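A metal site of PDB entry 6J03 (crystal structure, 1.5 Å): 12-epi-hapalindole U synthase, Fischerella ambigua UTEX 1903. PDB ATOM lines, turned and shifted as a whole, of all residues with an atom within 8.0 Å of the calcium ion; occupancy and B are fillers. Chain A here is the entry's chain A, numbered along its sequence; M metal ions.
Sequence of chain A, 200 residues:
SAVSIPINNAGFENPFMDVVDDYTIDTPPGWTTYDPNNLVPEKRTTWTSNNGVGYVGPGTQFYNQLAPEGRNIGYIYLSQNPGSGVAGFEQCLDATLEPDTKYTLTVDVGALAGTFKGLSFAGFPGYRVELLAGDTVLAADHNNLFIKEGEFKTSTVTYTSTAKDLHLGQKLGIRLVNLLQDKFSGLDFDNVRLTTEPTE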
ATOM      1  N   ASN A   9       4.279 -18.535 -18.105  1.00  0.00           N
ATOM      2  CA  ASN A   9       3.270 -19.584 -18.371  1.00  0.00           C
ATOM      3  C   ASN A   9       2.920 -20.279 -17.054  1.00  0.00           C
ATOM      4  O   ASN A   9       2.840 -21.529 -17.002  1.00  0.00           O
ATOM      5  CB  ASN A   9       3.736 -20.559 -19.454  1.00  0.00           C
ATOM      6  CG  ASN A   9       2.617 -21.306 -20.133  1.00  0.00           C
ATOM      7  OD1 ASN A   9       1.453 -20.922 -20.028  1.00  0.00           O
ATOM      8  ND2 ASN A   9       2.974 -22.370 -20.841  1.00  0.00           N
ATOM      9  N   ALA A  10       2.578 -19.484 -16.049  1.00  0.00           N
ATOM     10  CA  ALA A  10       2.430 -19.942 -14.658  1.00  0.00           C
ATOM     11  C   ALA A  10       1.216 -20.864 -14.499  1.00  0.00           C
ATOM     12  O   ALA A  10       1.173 -21.607 -13.525  1.00  0.00           O
ATOM     13  CB  ALA A  10       2.319 -18.762 -13.744  1.00  0.00           C
ATOM     14  N   GLY A  11       0.236 -20.753 -15.397  1.00  0.00           N
ATOM     15  CA  GLY A  11      -1.003 -21.531 -15.310  1.00  0.00           C
ATOM     16  C   GLY A  11      -1.119 -22.527 -16.447  1.00  0.00           C
ATOM     17  O   GLY A  11      -2.231 -23.053 -16.642  1.00  0.00           O
ATOM     18  N   PHE A  12      -0.055 -22.749 -17.206  1.00  0.00           N
ATOM     19  CA  PHE A  12      -0.060 -23.698 -18.353  1.00  0.00           C
ATOM     20  C   PHE A  12      -1.173 -23.316 -19.329  1.00  0.00           C
ATOM     21  O   PHE A  12      -1.634 -24.180 -20.082  1.00  0.00           O
ATOM     22  CB  PHE A  12      -0.191 -25.138 -17.862  1.00  0.00           C
ATOM     23  CG  PHE A  12       0.964 -25.567 -16.987  1.00  0.00           C
ATOM     24  CD1 PHE A  12       2.201 -25.847 -17.551  1.00  0.00           C
ATOM     25  CD2 PHE A  12       0.837 -25.580 -15.620  1.00  0.00           C
ATOM     26  CE1 PHE A  12       3.283 -26.164 -16.754  1.00  0.00           C
ATOM     27  CE2 PHE A  12       1.931 -25.871 -14.817  1.00  0.00           C
ATOM     28  CZ  PHE A  12       3.146 -26.147 -15.390  1.00  0.00           C
ATOM     29  N   GLU A  13      -1.472 -22.023 -19.432  1.00  0.00           N
ATOM     30  CA  GLU A  13      -2.568 -21.542 -20.306  1.00  0.00           C
ATOM     31  C   GLU A  13      -2.122 -21.469 -21.756  1.00  0.00           C
ATOM     32  O   GLU A  13      -2.973 -21.334 -22.641  1.00  0.00           O
ATOM     33  CB  GLU A  13      -3.072 -20.196 -19.820  1.00  0.00           C
ATOM     34  CG  GLU A  13      -3.758 -20.313 -18.479  1.00  0.00           C
ATOM     35  CD  GLU A  13      -4.961 -21.229 -18.542  1.00  0.00           C
ATOM     36  OE1 GLU A  13      -5.882 -20.934 -19.349  1.00  0.00           O
ATOM     37  OE2 GLU A  13      -4.988 -22.247 -17.784  1.00  0.00           O
ATOM     38  N   ASN A  14      -0.820 -21.546 -21.993  1.00  0.00           N
ATOM     39  CA  ASN A  14      -0.227 -21.532 -23.339  1.00  0.00           C
ATOM     40  C   ASN A  14       0.368 -22.902 -23.611  1.00  0.00           C
ATOM     41  O   ASN A  14       1.187 -23.374 -22.844  1.00  0.00           O
ATOM     42  CB  ASN A  14       0.822 -20.428 -23.417  1.00  0.00           C
ATOM     43  CG  ASN A  14       1.081 -19.981 -24.821  1.00  0.00           C
ATOM     44  OD1 ASN A  14       1.515 -20.794 -25.624  1.00  0.00           O
ATOM     45  ND2 ASN A  14       0.793 -18.706 -25.111  1.00  0.00           N
ATOM     46  N   GLY A  54      -3.351 -29.685 -20.813  1.00  0.00           N
ATOM     47  CA  GLY A  54      -4.675 -30.296 -21.031  1.00  0.00           C
ATOM     48  C   GLY A  54      -5.784 -29.335 -20.666  1.00  0.00           C
ATOM     49  O   GLY A  54      -5.674 -28.619 -19.671  1.00  0.00           O
ATOM     50  N   VAL A  56      -9.041 -28.569 -19.176  1.00  0.00           N
ATOM     51  CA  VAL A  56      -9.996 -29.089 -18.149  1.00  0.00           C
ATOM     52  C   VAL A  56     -11.139 -28.090 -18.022  1.00  0.00           C
ATOM     53  O   VAL A  56     -11.049 -27.172 -17.182  1.00  0.00           O
ATOM     54  CB  VAL A  56      -9.307 -29.381 -16.811  1.00  0.00           C
ATOM     55  CG1 VAL A  56     -10.300 -29.977 -15.824  1.00  0.00           C
ATOM     56  CG2 VAL A  56      -8.102 -30.299 -17.010  1.00  0.00           C
ATOM     57  N   ALA A  67     -10.235 -26.786 -14.230  1.00  0.00           N
ATOM     58  CA  ALA A  67      -8.842 -26.436 -13.917  1.00  0.00           C
ATOM     59  C   ALA A  67      -8.861 -25.527 -12.697  1.00  0.00           C
ATOM     60  O   ALA A  67      -9.726 -24.642 -12.589  1.00  0.00           O
ATOM     61  CB  ALA A  67      -8.187 -25.744 -15.075  1.00  0.00           C
ATOM     62  N   PRO A  68      -7.837 -25.606 -11.825  1.00  0.00           N
ATOM     63  CA  PRO A  68      -7.763 -24.669 -10.712  1.00  0.00           C
ATOM     64  C   PRO A  68      -7.789 -23.215 -11.196  1.00  0.00           C
ATOM     65  O   PRO A  68      -8.324 -22.344 -10.491  1.00  0.00           O
ATOM     66  CB  PRO A  68      -6.437 -25.038 -10.052  1.00  0.00           C
ATOM     67  CG  PRO A  68      -6.343 -26.534 -10.305  1.00  0.00           C
ATOM     68  CD  PRO A  68      -6.876 -26.704 -11.710  1.00  0.00           C
ATOM     69  N   GLU A  69      -7.150 -22.975 -12.333  1.00  0.00           N
ATOM     70  CA  GLU A  69      -6.987 -21.613 -12.885  1.00  0.00           C
ATOM     71  C   GLU A  69      -7.153 -21.700 -14.403  1.00  0.00           C
ATOM     72  O   GLU A  69      -6.562 -22.577 -15.048  1.00  0.00           O
ATOM     73  CB  GLU A  69      -5.617 -21.073 -12.451  1.00  0.00           C
ATOM     74  CG  GLU A  69      -5.270 -19.749 -13.064  1.00  0.00           C
ATOM     75  CD  GLU A  69      -4.713 -19.754 -14.471  1.00  0.00           C
ATOM     76  OE1 GLU A  69      -4.273 -20.827 -14.984  1.00  0.00           O
ATOM     77  OE2 GLU A  69      -4.775 -18.681 -15.085  1.00  0.00           O
ATOM     78  N   GLY A  70      -7.924 -20.776 -14.960  1.00  0.00           N
ATOM     79  CA  GLY A  70      -8.040 -20.673 -16.417  1.00  0.00           C
ATOM     80  C   GLY A  70      -8.625 -21.940 -17.017  1.00  0.00           C
ATOM     81  O   GLY A  70      -9.494 -22.586 -16.386  1.00  0.00           O
ATOM     82  N   ARG A  71      -8.161 -22.270 -18.217  1.00  0.00           N
ATOM     83  CA  ARG A  71      -8.683 -23.402 -19.029  1.00  0.00           C
ATOM     84  C   ARG A  71      -7.865 -24.657 -18.747  1.00  0.00           C
ATOM     85  O   ARG A  71      -8.436 -25.752 -18.846  1.00  0.00           O
ATOM     86  CB  ARG A  71      -8.612 -23.044 -20.508  1.00  0.00           C
ATOM     87  CG  ARG A  71      -9.518 -21.876 -20.857  1.00  0.00           C
ATOM     88  CD  ARG A  71      -9.314 -21.352 -22.258  1.00  0.00           C
ATOM     89  NE  ARG A  71      -9.688 -22.269 -23.319  1.00  0.00           N
ATOM     90  CZ  ARG A  71     -10.837 -22.202 -23.980  1.00  0.00           C
ATOM     91  NH1 ARG A  71     -11.805 -21.399 -23.572  1.00  0.00           N
ATOM     92  NH2 ARG A  71     -11.026 -22.970 -25.034  1.00  0.00           N
ATOM     93  N   ASN A  72      -6.553 -24.519 -18.572  1.00  0.00           N
ATOM     94  CA  ASN A  72      -5.625 -25.642 -18.747  1.00  0.00           C
ATOM     95  C   ASN A  72      -4.917 -26.023 -17.462  1.00  0.00           C
ATOM     96  O   ASN A  72      -4.711 -25.185 -16.570  1.00  0.00           O
ATOM     97  CB  ASN A  72      -4.504 -25.329 -19.725  1.00  0.00           C
ATOM     98  CG  ASN A  72      -4.923 -25.090 -21.157  1.00  0.00           C
ATOM     99  OD1 ASN A  72      -6.057 -25.360 -21.561  1.00  0.00           O
ATOM    100  ND2 ASN A  72      -3.965 -24.554 -21.911  1.00  0.00           N
ATOM    101  N   ILE A  73      -4.474 -27.267 -17.425  1.00  0.00           N
ATOM    102  CA  ILE A  73      -3.457 -27.737 -16.464  1.00  0.00           C
ATOM    103  C   ILE A  73      -2.212 -28.140 -17.254  1.00  0.00           C
ATOM    104  O   ILE A  73      -2.284 -28.283 -18.502  1.00  0.00           O
ATOM    105  CB  ILE A  73      -4.033 -28.855 -15.572  1.00  0.00           C
ATOM    106  CG1 ILE A  73      -4.449 -30.116 -16.341  1.00  0.00           C
ATOM    107  CG2 ILE A  73      -5.203 -28.323 -14.776  1.00  0.00           C
ATOM    108  CD1 ILE A  73      -3.305 -30.955 -16.888  1.00  0.00           C
ATOM    109  N   GLY A  74      -1.111 -28.309 -16.544  1.00  0.00           N
ATOM    110  CA  GLY A  74       0.099 -28.933 -17.110  1.00  0.00           C
ATOM    111  C   GLY A  74       0.235 -30.333 -16.563  1.00  0.00           C
ATOM    112  O   GLY A  74       0.041 -30.528 -15.365  1.00  0.00           O
ATOM    113  N   ASP A 108      -1.082 -25.898  -7.407  1.00  0.00           N
ATOM    114  CA  ASP A 108      -2.172 -26.882  -7.296  1.00  0.00           C
ATOM    115  C   ASP A 108      -1.715 -28.183  -7.963  1.00  0.00           C
ATOM    116  O   ASP A 108      -1.071 -28.148  -9.020  1.00  0.00           O
ATOM    117  CB  ASP A 108      -3.470 -26.317  -7.880  1.00  0.00           C
ATOM    118  CG  ASP A 108      -3.947 -25.066  -7.168  1.00  0.00           C
ATOM    119  OD1 ASP A 108      -3.764 -24.995  -5.960  1.00  0.00           O
ATOM    120  OD2 ASP A 108      -4.237 -24.082  -7.878  1.00  0.00           O
ATOM    121  N   PHE A 189      -0.398 -30.298 -12.650  1.00  0.00           N
ATOM    122  CA  PHE A 189      -0.086 -29.079 -11.876  1.00  0.00           C
ATOM    123  C   PHE A 189      -0.815 -27.885 -12.470  1.00  0.00           C
ATOM    124  O   PHE A 189      -1.084 -27.865 -13.689  1.00  0.00           O
ATOM    125  CB  PHE A 189       1.413 -28.805 -11.910  1.00  0.00           C
ATOM    126  CG  PHE A 189       2.236 -29.875 -11.239  1.00  0.00           C
ATOM    127  CD1 PHE A 189       2.392 -29.893  -9.864  1.00  0.00           C
ATOM    128  CD2 PHE A 189       2.838 -30.859 -11.993  1.00  0.00           C
ATOM    129  CE1 PHE A 189       3.166 -30.878  -9.263  1.00  0.00           C
ATOM    130  CE2 PHE A 189       3.632 -31.834 -11.394  1.00  0.00           C
ATOM    131  CZ  PHE A 189       3.792 -31.832 -10.032  1.00  0.00           C
ATOM    132  N   ASP A 190      -1.094 -26.873 -11.648  1.00  0.00           N
ATOM    133  CA  ASP A 190      -1.652 -25.609 -12.170  1.00  0.00           C
ATOM    134  C   ASP A 190      -1.350 -24.480 -11.204  1.00  0.00           C
ATOM    135  O   ASP A 190      -1.021 -24.750 -10.025  1.00  0.00           O
ATOM    136  CB  ASP A 190      -3.156 -25.724 -12.409  1.00  0.00           C
ATOM    137  CG  ASP A 190      -3.739 -24.663 -13.331  1.00  0.00           C
ATOM    138  OD1 ASP A 190      -2.943 -23.921 -13.969  1.00  0.00           O
ATOM    139  OD2 ASP A 190      -4.970 -24.642 -13.477  1.00  0.00           O
ATOM    140  N   ASN A 191      -1.422 -23.265 -11.707  1.00  0.00           N
ATOM    141  CA  ASN A 191      -1.520 -22.045 -10.884  1.00  0.00           C
ATOM    142  C   ASN A 191      -0.283 -21.931  -9.995  1.00  0.00           C
ATOM    143  O   ASN A 191      -0.417 -21.846  -8.772  1.00  0.00           O
ATOM    144  CB  ASN A 191      -2.828 -22.013 -10.098  1.00  0.00           C
ATOM    145  CG  ASN A 191      -3.107 -20.662  -9.484  1.00  0.00           C
ATOM    146  OD1 ASN A 191      -2.597 -19.645  -9.945  1.00  0.00           O
ATOM    147  ND2 ASN A 191      -3.919 -20.660  -8.435  1.00  0.00           N
ATOM    148  N   VAL A 192       0.894 -21.876 -10.620  1.00  0.00           N
ATOM    149  CA  VAL A 192       2.167 -21.710  -9.883  1.00  0.00           C
ATOM    150  C   VAL A 192       2.285 -20.257  -9.424  1.00  0.00           C
ATOM    151  O   VAL A 192       2.115 -19.346 -10.251  1.00  0.00           O
ATOM    152  CB  VAL A 192       3.368 -22.137 -10.730  1.00  0.00           C
ATOM    153  CG1 VAL A 192       4.628 -22.150  -9.911  1.00  0.00           C
ATOM    154  CG2 VAL A 192       3.126 -23.499 -11.378  1.00  0.00           C
HETATM  155 CA    CA M   1      -4.402 -23.080 -15.648  1.00  0.00          CA
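The side-chain carboxylate (OE1) of Glu 13 lies within hydrogen-bond range of the backbone NH (N) of Arg 71.
ND2 of Asn 72 is in hydrogen-bond range of O of Phe 12 (3.0 Å).
O of Asp 190 lies within hydrogen-bond range of N of Asp 108 (2.9 Å).
N of Glu 13 sits at hydrogen-bond distance from OD1 of Asn 9, at 3.2 Å.
Of the 21 residues printed, 5 come within 4 Å of the calcium ion.
The nearest printed residue that does not touch the calcium ion is Gly 70 (4.3 Å).
The calcium ion is bound by the backbone carbonyl oxygen (O) of Glu 69 (2.3 Å), the backbone carbonyl oxygen (O) of Asn 72 (2.3 Å), the side-chain carboxylate (OE1) of Glu 69 (2.4 Å), the side-chain carboxylate (OE2) of Glu 13 (2.4 Å), the side-chain carboxylate (OD1) of Asp 190 (2.4 Å), the backbone carbonyl oxygen (O) of Gly 11 (2.4 Å) and the side-chain carboxylate (OD2) of Asp 190 (2.7 Å).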
